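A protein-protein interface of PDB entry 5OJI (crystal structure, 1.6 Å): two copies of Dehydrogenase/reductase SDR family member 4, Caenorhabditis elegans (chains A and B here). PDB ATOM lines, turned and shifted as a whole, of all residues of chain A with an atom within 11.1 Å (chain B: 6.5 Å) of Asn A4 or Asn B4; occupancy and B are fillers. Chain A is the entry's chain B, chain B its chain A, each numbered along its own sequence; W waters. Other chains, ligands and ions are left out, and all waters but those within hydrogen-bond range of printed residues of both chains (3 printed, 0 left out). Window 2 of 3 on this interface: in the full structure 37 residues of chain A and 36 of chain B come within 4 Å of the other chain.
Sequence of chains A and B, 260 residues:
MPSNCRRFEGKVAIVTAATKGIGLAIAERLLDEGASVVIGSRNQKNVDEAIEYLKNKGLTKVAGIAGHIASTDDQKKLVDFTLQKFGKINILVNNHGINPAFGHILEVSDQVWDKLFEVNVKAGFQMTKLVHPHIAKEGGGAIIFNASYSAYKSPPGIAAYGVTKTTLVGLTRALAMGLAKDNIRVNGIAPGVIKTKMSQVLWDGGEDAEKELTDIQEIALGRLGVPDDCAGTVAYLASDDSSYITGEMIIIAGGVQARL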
ATOM      1  N   MET A   1     -16.190 -23.550   3.030  1.00  0.00           N
ATOM      2  CA  MET A   1     -17.301 -23.440   2.042  1.00  0.00           C
ATOM      3  C   MET A   1     -17.218 -22.101   1.308  1.00  0.00           C
ATOM      4  O   MET A   1     -16.623 -21.147   1.818  1.00  0.00           O
ATOM      5  CB  MET A   1     -18.660 -23.567   2.743  1.00  0.00           C
ATOM      6  CG  MET A   1     -19.828 -23.878   1.807  1.00  0.00           C
ATOM      7  SD  MET A   1     -21.443 -23.431   2.482  1.00  0.00           S
ATOM      8  CE  MET A   1     -22.461 -23.560   1.009  1.00  0.00           C
ATOM      9  N   PRO A   2     -17.777 -22.028   0.102  1.00  0.00           N
ATOM     10  CA  PRO A   2     -18.078 -20.728  -0.498  1.00  0.00           C
ATOM     11  C   PRO A   2     -19.489 -20.276  -0.160  1.00  0.00           C
ATOM     12  O   PRO A   2     -20.388 -21.074   0.121  1.00  0.00           O
ATOM     13  CB  PRO A   2     -17.953 -20.986  -2.010  1.00  0.00           C
ATOM     14  CG  PRO A   2     -17.419 -22.378  -2.147  1.00  0.00           C
ATOM     15  CD  PRO A   2     -17.832 -23.093  -0.910  1.00  0.00           C
ATOM     16  N   SER A   3     -19.664 -18.962  -0.194  1.00  0.00           N
ATOM     17  CA  SER A   3     -20.982 -18.357  -0.133  1.00  0.00           C
ATOM     18  C   SER A   3     -21.513 -17.996  -1.512  1.00  0.00           C
ATOM     19  O   SER A   3     -22.733 -17.858  -1.681  1.00  0.00           O
ATOM     20  CB  SER A   3     -20.936 -17.098   0.736  1.00  0.00           C
ATOM     21  OG  SER A   3     -20.107 -16.123   0.138  1.00  0.00           O
ATOM     22  N   ASN A   4     -20.615 -17.866  -2.492  1.00  0.00           N
ATOM     23  CA  ASN A   4     -20.873 -17.300  -3.812  1.00  0.00           C
ATOM     24  C   ASN A   4     -21.240 -15.825  -3.752  1.00  0.00           C
ATOM     25  O   ASN A   4     -21.529 -15.217  -4.794  1.00  0.00           O
ATOM     26  CB  ASN A   4     -21.955 -18.083  -4.566  1.00  0.00           C
ATOM     27  CG  ASN A   4     -21.372 -19.212  -5.390  1.00  0.00           C
ATOM     28  OD1 ASN A   4     -21.220 -19.093  -6.605  1.00  0.00           O
ATOM     29  ND2 ASN A   4     -21.009 -20.303  -4.725  1.00  0.00           N
ATOM     30  N   CYS A   5     -21.224 -15.222  -2.563  1.00  0.00           N
ATOM     31  CA  CYS A   5     -21.467 -13.793  -2.465  1.00  0.00           C
ATOM     32  C   CYS A   5     -20.454 -13.028  -3.310  1.00  0.00           C
ATOM     33  O   CYS A   5     -19.267 -13.358  -3.333  1.00  0.00           O
ATOM     34  CB  CYS A   5     -21.383 -13.335  -1.010  1.00  0.00           C
ATOM     35  SG  CYS A   5     -22.669 -13.974   0.126  1.00  0.00           S
ATOM     36  N   ARG A   6     -20.939 -12.012  -4.027  1.00  0.00           N
ATOM     37  CA  ARG A   6     -20.102 -11.105  -4.816  1.00  0.00           C
ATOM     38  C   ARG A   6     -20.579  -9.674  -4.605  1.00  0.00           C
ATOM     39  O   ARG A   6     -21.065  -9.006  -5.513  1.00  0.00           O
ATOM     40  CB  ARG A   6     -20.157 -11.404  -6.312  1.00  0.00           C
ATOM     41  CG  ARG A   6     -19.627 -12.734  -6.732  1.00  0.00           C
ATOM     42  CD  ARG A   6     -18.105 -12.767  -6.732  1.00  0.00           C
ATOM     43  NE  ARG A   6     -17.486 -11.896  -7.739  1.00  0.00           N
ATOM     44  CZ  ARG A   6     -16.173 -11.856  -7.962  1.00  0.00           C
ATOM     45  NH1 ARG A   6     -15.363 -12.629  -7.253  1.00  0.00           N
ATOM     46  NH2 ARG A   6     -15.658 -11.046  -8.882  1.00  0.00           N
ATOM     47  N   ARG A   7     -20.440  -9.177  -3.392  1.00  0.00           N
ATOM     48  CA  ARG A   7     -21.013  -7.882  -3.067  1.00  0.00           C
ATOM     49  C   ARG A   7     -20.038  -6.715  -3.255  1.00  0.00           C
ATOM     50  O   ARG A   7     -20.440  -5.562  -3.057  1.00  0.00           O
ATOM     51  CB  ARG A   7     -21.533  -7.916  -1.629  1.00  0.00           C
ATOM     52  CG  ARG A   7     -22.713  -8.886  -1.441  1.00  0.00           C
ATOM     53  CD  ARG A   7     -23.055  -9.065   0.026  1.00  0.00           C
ATOM     54  NE  ARG A   7     -22.011  -9.787   0.722  1.00  0.00           N
ATOM     55  CZ  ARG A   7     -22.126 -10.276   1.950  1.00  0.00           C
ATOM     56  NH1 ARG A   7     -23.257 -10.141   2.635  1.00  0.00           N
ATOM     57  NH2 ARG A   7     -21.111 -10.939   2.478  1.00  0.00           N
ATOM     58  N   PHE A   8     -18.791  -6.966  -3.680  1.00  0.00           N
ATOM     59  CA  PHE A   8     -17.757  -5.935  -3.629  1.00  0.00           C
ATOM     60  C   PHE A   8     -17.074  -5.670  -4.967  1.00  0.00           C
ATOM     61  O   PHE A   8     -15.983  -5.090  -4.988  1.00  0.00           O
ATOM     62  CB  PHE A   8     -16.719  -6.307  -2.570  1.00  0.00           C
ATOM     63  CG  PHE A   8     -17.270  -6.266  -1.177  1.00  0.00           C
ATOM     64  CD1 PHE A   8     -17.281  -5.078  -0.460  1.00  0.00           C
ATOM     65  CD2 PHE A   8     -17.827  -7.399  -0.609  1.00  0.00           C
ATOM     66  CE1 PHE A   8     -17.818  -5.022   0.811  1.00  0.00           C
ATOM     67  CE2 PHE A   8     -18.366  -7.352   0.671  1.00  0.00           C
ATOM     68  CZ  PHE A   8     -18.354  -6.163   1.386  1.00  0.00           C
ATOM     69  N   GLU A   9     -17.684  -6.034  -6.088  1.00  0.00           N
ATOM     70  CA  GLU A   9     -17.051  -5.742  -7.367  1.00  0.00           C
ATOM     71  C   GLU A   9     -16.928  -4.234  -7.551  1.00  0.00           C
ATOM     72  O   GLU A   9     -17.859  -3.470  -7.267  1.00  0.00           O
ATOM     73  CB  GLU A   9     -17.831  -6.391  -8.516  1.00  0.00           C
ATOM     74  CG  GLU A   9     -17.711  -7.899  -8.484  1.00  0.00           C
ATOM     75  CD  GLU A   9     -18.433  -8.596  -9.613  1.00  0.00           C
ATOM     76  OE1 GLU A   9     -18.264  -9.830  -9.745  1.00  0.00           O
ATOM     77  OE2 GLU A   9     -19.158  -7.917 -10.367  1.00  0.00           O
ATOM     78  N   GLU A  28      -9.179 -12.079   2.548  1.00  0.00           N
ATOM     79  CA  GLU A  28      -9.496 -13.156   1.628  1.00  0.00           C
ATOM     80  C   GLU A  28     -10.972 -13.137   1.252  1.00  0.00           C
ATOM     81  O   GLU A  28     -11.322 -13.349   0.090  1.00  0.00           O
ATOM     82  CB  GLU A  28      -9.123 -14.506   2.238  1.00  0.00           C
ATOM     83  CG  GLU A  28      -9.293 -15.647   1.242  1.00  0.00           C
ATOM     84  CD  GLU A  28      -8.834 -16.995   1.771  1.00  0.00           C
ATOM     85  OE1 GLU A  28      -8.073 -17.032   2.758  1.00  0.00           O
ATOM     86  OE2 GLU A  28      -9.233 -18.022   1.182  1.00  0.00           O
ATOM     87  N   ARG A  29     -11.854 -12.890   2.230  1.00  0.00           N
ATOM     88  CA  ARG A  29     -13.292 -12.895   1.960  1.00  0.00           C
ATOM     89  C   ARG A  29     -13.687 -11.730   1.052  1.00  0.00           C
ATOM     90  O   ARG A  29     -14.458 -11.908   0.102  1.00  0.00           O
ATOM     91  CB  ARG A  29     -14.065 -12.876   3.288  1.00  0.00           C
ATOM     92  CG  ARG A  29     -15.585 -12.729   3.134  1.00  0.00           C
ATOM     93  CD  ARG A  29     -16.190 -13.823   2.247  1.00  0.00           C
ATOM     94  NE  ARG A  29     -17.640 -13.658   2.127  1.00  0.00           N
ATOM     95  CZ  ARG A  29     -18.557 -14.278   2.869  1.00  0.00           C
ATOM     96  NH1 ARG A  29     -19.841 -14.013   2.652  1.00  0.00           N
ATOM     97  NH2 ARG A  29     -18.215 -15.164   3.804  1.00  0.00           N
ATOM     98  N   LEU A  30     -13.131 -10.538   1.291  1.00  0.00           N
ATOM     99  CA  LEU A  30     -13.434  -9.411   0.419  1.00  0.00           C
ATOM    100  C   LEU A  30     -12.956  -9.677  -1.005  1.00  0.00           C
ATOM    101  O   LEU A  30     -13.663  -9.369  -1.975  1.00  0.00           O
ATOM    102  CB  LEU A  30     -12.815  -8.137   0.990  1.00  0.00           C
ATOM    103  CG  LEU A  30     -13.393  -7.761   2.355  1.00  0.00           C
ATOM    104  CD1 LEU A  30     -12.662  -6.550   2.911  1.00  0.00           C
ATOM    105  CD2 LEU A  30     -14.903  -7.465   2.267  1.00  0.00           C
ATOM    106  N   LEU A  31     -11.757 -10.237  -1.147  1.00  0.00           N
ATOM    107  CA  LEU A  31     -11.254 -10.601  -2.466  1.00  0.00           C
ATOM    108  C   LEU A  31     -12.157 -11.640  -3.117  1.00  0.00           C
ATOM    109  O   LEU A  31     -12.460 -11.549  -4.311  1.00  0.00           O
ATOM    110  CB  LEU A  31      -9.819 -11.129  -2.350  1.00  0.00           C
ATOM    111  CG  LEU A  31      -8.723 -10.079  -2.054  1.00  0.00           C
ATOM    112  CD1 LEU A  31      -7.433 -10.724  -1.483  1.00  0.00           C
ATOM    113  CD2 LEU A  31      -8.407  -9.251  -3.297  1.00  0.00           C
ATOM    114  N   ASP A  32     -12.599 -12.637  -2.349  1.00  0.00           N
ATOM    115  CA  ASP A  32     -13.499 -13.630  -2.916  1.00  0.00           C
ATOM    116  C   ASP A  32     -14.786 -12.989  -3.434  1.00  0.00           C
ATOM    117  O   ASP A  32     -15.363 -13.484  -4.403  1.00  0.00           O
ATOM    118  CB  ASP A  32     -13.799 -14.720  -1.883  1.00  0.00           C
ATOM    119  CG  ASP A  32     -14.421 -15.954  -2.509  1.00  0.00           C
ATOM    120  OD1 ASP A  32     -13.798 -16.534  -3.421  1.00  0.00           O
ATOM    121  OD2 ASP A  32     -15.532 -16.331  -2.095  1.00  0.00           O
ATOM    122  N   GLU A  33     -15.226 -11.874  -2.839  1.00  0.00           N
ATOM    123  CA  GLU A  33     -16.454 -11.200  -3.244  1.00  0.00           C
ATOM    124  C   GLU A  33     -16.240 -10.116  -4.294  1.00  0.00           C
ATOM    125  O   GLU A  33     -17.191  -9.388  -4.610  1.00  0.00           O
ATOM    126  CB  GLU A  33     -17.148 -10.606  -2.025  1.00  0.00           C
ATOM    127  CG  GLU A  33     -17.650 -11.676  -1.083  1.00  0.00           C
ATOM    128  CD  GLU A  33     -18.865 -11.249  -0.287  1.00  0.00           C
ATOM    129  OE1 GLU A  33     -19.681 -10.432  -0.777  1.00  0.00           O
ATOM    130  OE2 GLU A  33     -18.994 -11.732   0.849  1.00  0.00           O
ATOM    131  N   GLY A  34     -15.032 -10.006  -4.858  1.00  0.00           N
ATOM    132  CA  GLY A  34     -14.769  -9.113  -5.967  1.00  0.00           C
ATOM    133  C   GLY A  34     -13.997  -7.860  -5.630  1.00  0.00           C
ATOM    134  O   GLY A  34     -13.717  -7.063  -6.532  1.00  0.00           O
ATOM    135  N   ALA A  35     -13.621  -7.664  -4.374  1.00  0.00           N
ATOM    136  CA  ALA A  35     -12.954  -6.430  -4.001  1.00  0.00           C
ATOM    137  C   ALA A  35     -11.507  -6.410  -4.491  1.00  0.00           C
ATOM    138  O   ALA A  35     -10.890  -7.447  -4.769  1.00  0.00           O
ATOM    139  CB  ALA A  35     -12.971  -6.251  -2.484  1.00  0.00           C
ATOM    140  N   GLY A 232     -17.194 -13.412   7.545  1.00  0.00           N
ATOM    141  CA  GLY A 232     -18.540 -13.193   7.045  1.00  0.00           C
ATOM    142  C   GLY A 232     -19.194 -11.968   7.650  1.00  0.00           C
ATOM    143  O   GLY A 232     -19.952 -11.260   6.984  1.00  0.00           O
ATOM    144  N   ALA A 235     -17.573  -8.781   6.073  1.00  0.00           N
ATOM    145  CA  ALA A 235     -18.092  -8.616   4.723  1.00  0.00           C
ATOM    146  C   ALA A 235     -19.522  -8.082   4.757  1.00  0.00           C
ATOM    147  O   ALA A 235     -19.864  -7.140   4.038  1.00  0.00           O
ATOM    148  CB  ALA A 235     -18.021  -9.945   3.970  1.00  0.00           C
ATOM    149  N   SER A 239     -20.857  -4.386   3.355  1.00  0.00           N
ATOM    150  CA  SER A 239     -21.689  -4.495   2.164  1.00  0.00           C
ATOM    151  C   SER A 239     -22.975  -3.701   2.317  1.00  0.00           C
ATOM    152  O   SER A 239     -23.313  -3.190   3.386  1.00  0.00           O
ATOM    153  CB  SER A 239     -22.036  -5.960   1.885  1.00  0.00           C
ATOM    154  OG  SER A 239     -23.006  -6.404   2.820  1.00  0.00           O
ATOM    155  N   ASP A 240     -23.722  -3.633   1.218  1.00  0.00           N
ATOM    156  CA  ASP A 240     -25.039  -3.022   1.249  1.00  0.00           C
ATOM    157  C   ASP A 240     -26.070  -3.862   2.003  1.00  0.00           C
ATOM    158  O   ASP A 240     -27.195  -3.392   2.191  1.00  0.00           O
ATOM    159  CB  ASP A 240     -25.503  -2.756  -0.182  1.00  0.00           C
ATOM    160  CG  ASP A 240     -24.702  -1.642  -0.859  1.00  0.00           C
ATOM    161  OD1 ASP A 240     -24.032  -0.858  -0.152  1.00  0.00           O
ATOM    162  OD2 ASP A 240     -24.741  -1.551  -2.101  1.00  0.00           O
ATOM    163  N   ASP A 241     -25.724  -5.074   2.443  1.00  0.00           N
ATOM    164  CA  ASP A 241     -26.645  -5.841   3.276  1.00  0.00           C
ATOM    165  C   ASP A 241     -26.835  -5.218   4.652  1.00  0.00           C
ATOM    166  O   ASP A 241     -27.761  -5.613   5.366  1.00  0.00           O
ATOM    167  CB  ASP A 241     -26.165  -7.286   3.428  1.00  0.00           C
ATOM    168  CG  ASP A 241     -26.403  -8.118   2.172  1.00  0.00           C
ATOM    169  OD1 ASP A 241     -27.119  -7.639   1.284  1.00  0.00           O
ATOM    170  OD2 ASP A 241     -25.858  -9.235   2.057  1.00  0.00           O
ATOM    171  N   MET B   1     -28.567  -4.447  -5.312  1.00  0.00           N
ATOM    172  CA  MET B   1     -29.568  -5.278  -4.591  1.00  0.00           C
ATOM    173  C   MET B   1     -29.129  -6.745  -4.653  1.00  0.00           C
ATOM    174  O   MET B   1     -28.812  -7.320  -3.615  1.00  0.00           O
ATOM    175  CB  MET B   1     -30.982  -5.045  -5.161  1.00  0.00           C
ATOM    176  CG  MET B   1     -31.939  -6.241  -5.148  1.00  0.00           C
ATOM    177  SD  MET B   1     -33.679  -5.734  -5.240  1.00  0.00           S
ATOM    178  CE  MET B   1     -33.678  -4.674  -6.693  1.00  0.00           C
ATOM    179  N   PRO B   2     -29.050  -7.350  -5.841  1.00  0.00           N
ATOM    180  CA  PRO B   2     -28.617  -8.752  -5.894  1.00  0.00           C
ATOM    181  C   PRO B   2     -27.203  -8.902  -5.351  1.00  0.00           C
ATOM    182  O   PRO B   2     -26.322  -8.080  -5.614  1.00  0.00           O
ATOM    183  CB  PRO B   2     -28.701  -9.101  -7.387  1.00  0.00           C
ATOM    184  CG  PRO B   2     -29.584  -8.042  -7.986  1.00  0.00           C
ATOM    185  CD  PRO B   2     -29.267  -6.815  -7.195  1.00  0.00           C
ATOM    186  N   SER B   3     -26.999  -9.961  -4.568  1.00  0.00           N
ATOM    187  CA  SER B   3     -25.722 -10.223  -3.927  1.00  0.00           C
ATOM    188  C   SER B   3     -24.991 -11.407  -4.534  1.00  0.00           C
ATOM    189  O   SER B   3     -23.818 -11.629  -4.203  1.00  0.00           O
ATOM    190  CB  SER B   3     -25.941 -10.483  -2.430  1.00  0.00           C
ATOM    191  OG  SER B   3     -26.500 -11.778  -2.221  1.00  0.00           O
ATOM    192  N   ASN B   4     -25.660 -12.182  -5.390  1.00  0.00           N
ATOM    193  CA  ASN B   4     -25.171 -13.475  -5.860  1.00  0.00           C
ATOM    194  C   ASN B   4     -24.909 -14.435  -4.708  1.00  0.00           C
ATOM    195  O   ASN B   4     -24.425 -15.552  -4.927  1.00  0.00           O
ATOM    196  CB  ASN B   4     -23.911 -13.305  -6.712  1.00  0.00           C
ATOM    197  CG  ASN B   4     -24.232 -12.897  -8.132  1.00  0.00           C
ATOM    198  OD1 ASN B   4     -24.122 -11.726  -8.497  1.00  0.00           O
ATOM    199  ND2 ASN B   4     -24.663 -13.862  -8.939  1.00  0.00           N
ATOM    200  N   CYS B   5     -25.250 -14.031  -3.482  1.00  0.00           N
ATOM    201  CA  CYS B   5     -25.159 -14.952  -2.363  1.00  0.00           C
ATOM    202  C   CYS B   5     -26.128 -16.099  -2.607  1.00  0.00           C
ATOM    203  O   CYS B   5     -27.273 -15.880  -3.011  1.00  0.00           O
ATOM    204  CB  CYS B   5     -25.494 -14.252  -1.041  1.00  0.00           C
ATOM    205  SG  CYS B   5     -24.326 -12.961  -0.463  1.00  0.00           S
ATOM    206  N   ARG B   6     -25.658 -17.322  -2.398  1.00  0.00           N
ATOM    207  CA  ARG B   6     -26.500 -18.510  -2.502  1.00  0.00           C
ATOM    208  C   ARG B   6     -26.243 -19.366  -1.279  1.00  0.00           C
ATOM    209  O   ARG B   6     -25.797 -20.509  -1.368  1.00  0.00           O
ATOM    210  CB  ARG B   6     -26.233 -19.321  -3.770  1.00  0.00           C
ATOM    211  CG  ARG B   6     -26.524 -18.590  -5.055  1.00  0.00           C
ATOM    212  CD  ARG B   6     -28.015 -18.471  -5.320  1.00  0.00           C
ATOM    213  NE  ARG B   6     -28.656 -19.762  -5.547  1.00  0.00           N
ATOM    214  CZ  ARG B   6     -29.931 -19.906  -5.899  1.00  0.00           C
ATOM    215  NH1 ARG B   6     -30.697 -18.837  -6.072  1.00  0.00           N
ATOM    216  NH2 ARG B   6     -30.443 -21.117  -6.078  1.00  0.00           N
ATOM    217  N   ARG B   7     -26.507 -18.788  -0.114  1.00  0.00           N
ATOM    218  CA  ARG B   7     -26.127 -19.440   1.120  1.00  0.00           C
ATOM    219  C   ARG B   7     -27.189 -20.399   1.631  1.00  0.00           C
ATOM    220  O   ARG B   7     -26.980 -21.024   2.676  1.00  0.00           O
ATOM    221  CB  ARG B   7     -25.814 -18.385   2.186  1.00  0.00           C
ATOM    222  CG  ARG B   7     -24.618 -17.508   1.820  1.00  0.00           C
ATOM    223  CD  ARG B   7     -24.464 -16.312   2.756  1.00  0.00           C
ATOM    224  NE  ARG B   7     -25.550 -15.350   2.617  1.00  0.00           N
ATOM    225  CZ  ARG B   7     -25.584 -14.167   3.220  1.00  0.00           C
ATOM    226  NH1 ARG B   7     -24.574 -13.779   3.998  1.00  0.00           N
ATOM    227  NH2 ARG B   7     -26.625 -13.366   3.042  1.00  0.00           N
ATOM    228  N   ASP B  32     -34.212 -15.781  -2.899  1.00  0.00           N
ATOM    229  CA  ASP B  32     -33.149 -15.368  -3.807  1.00  0.00           C
ATOM    230  C   ASP B  32     -31.874 -16.167  -3.592  1.00  0.00           C
ATOM    231  O   ASP B  32     -31.129 -16.405  -4.547  1.00  0.00           O
ATOM    232  CB  ASP B  32     -32.866 -13.881  -3.628  1.00  0.00           C
ATOM    233  CG  ASP B  32     -31.868 -13.365  -4.639  1.00  0.00           C
ATOM    234  OD1 ASP B  32     -32.166 -13.467  -5.848  1.00  0.00           O
ATOM    235  OD2 ASP B  32     -30.793 -12.877  -4.226  1.00  0.00           O
ATOM    236  N   GLU B  33     -31.592 -16.570  -2.354  1.00  0.00           N
ATOM    237  CA  GLU B  33     -30.379 -17.301  -2.030  1.00  0.00           C
ATOM    238  C   GLU B  33     -30.564 -18.808  -2.087  1.00  0.00           C
ATOM    239  O   GLU B  33     -29.668 -19.546  -1.659  1.00  0.00           O
ATOM    240  CB  GLU B  33     -29.874 -16.889  -0.646  1.00  0.00           C
ATOM    241  CG  GLU B  33     -29.466 -15.424  -0.605  1.00  0.00           C
ATOM    242  CD  GLU B  33     -28.375 -15.139   0.414  1.00  0.00           C
ATOM    243  OE1 GLU B  33     -27.561 -16.039   0.709  1.00  0.00           O
ATOM    244  OE2 GLU B  33     -28.359 -14.006   0.926  1.00  0.00           O
HETATM  245  O   HOH W   1     -22.564  -9.783  -7.799  1.00  0.00           O
HETATM  246  O   HOH W   2     -26.056 -10.816   4.308  1.00  0.00           O
HETATM  247  O   HOH W   3     -21.932 -12.120   5.106  1.00  0.00           O
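Ser A3 touches Arg B6, and with the chains exchanged Arg A6 touches Ser B3.
Ser A3 touches Arg B7, and with the chains exchanged Arg A7 touches Ser B3.
Cys A5 touches Asn B4, but with the chains exchanged Asn A4 does not touch Cys B5 (4.1 Å).
Cys A5 touches Arg B7, but with the chains exchanged Arg A7 does not touch Cys B5 (4.1 Å).
Positions printed for both chains: 1, 2, 3, 4, 5, 6, 7, 32 and 33.
Of the 10 pairs that touch across the chains among the printed residues, 8 have their exchanged pair printed and touching as well.
O of Ser B3 is in hydrogen-bond range of N of Arg A6 (2.9 Å).
The side-chain sulfur of Cys B5 forms a disulfide with the side-chain sulfur of Cys A5.
The backbone carbonyl oxygen (O) of Ser A3 is in hydrogen-bond range of the backbone NH (N) of Arg B6, 3.1 Å away.
O of Asn A4 lies close to O of Asn B4.
Of chain B, only Asn B4 comes within 4 Å of Asn A4.
Of the printed residues of chain A, Asn B4 touches Asn A4 (2.9 Å) and Cys A5 (3.99 Å).
No residue of chain A comes within 4 Å of Pro B2.
Cys B5 touches just these residues of chain A: Ser A3 and Cys A5.
Printed residues of chain A within 4 Å of Arg B7: Ser A3 and Cys A5.
Printed residues of chain B within 4 Å of Arg A6: Ser B3 (2.9 Å).
Along chain B the printed residues that touch a printed residue of chain A span positions 3 to 7.
Cys B5 touches Ser A3 (CA to O, 3.8 Å).
Arg B7 touches Ser A3 (CG to CB, 3.9 Å).
Ser B3 touches Cys A5.
Asn B4 touches Cys A5 (O to N, 3.99 Å).
Cys A5 touches Arg B7.
Arg A7 touches Ser B3 (CG to CB, 3.7 Å).
The side-chain hydroxyl (OG) of Ser B3 lies close to the backbone NH (N) of Cys B5 (2.9 Å).
NH1 of Arg B6 lies within hydrogen-bond range of O of Asp B32 (2.9 Å).
The guanidinium group of Arg B7 is in salt-bridge range of the side-chain carboxylate of Glu B33, at 2.8 Å.
The side-chain sulfur of Cys A5 is in hydrogen-bond range of the guanidinium group of Arg A29 (3.8 Å).
NH1 of Arg A6 is in hydrogen-bond range of O of Asp A32 (3.0 Å).
NH2 of Arg A7 is in salt-bridge range of OE2 of Glu A33 (2.8 Å).
Water W1 lies within hydrogen-bond range of OD1 of Asn B4 (2.6 Å) and O of Arg A6 (2.8 Å).
Water W2 lies within hydrogen-bond range of OD2 of Asp A241, NH2 of Arg B7 and NH1 of Arg A7.
Water W3 lies within hydrogen-bond range of O of Gly A232 (2.9 Å), NH2 of Arg A7 (3.0 Å) and NH1 of Arg B7 (3.3 Å).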
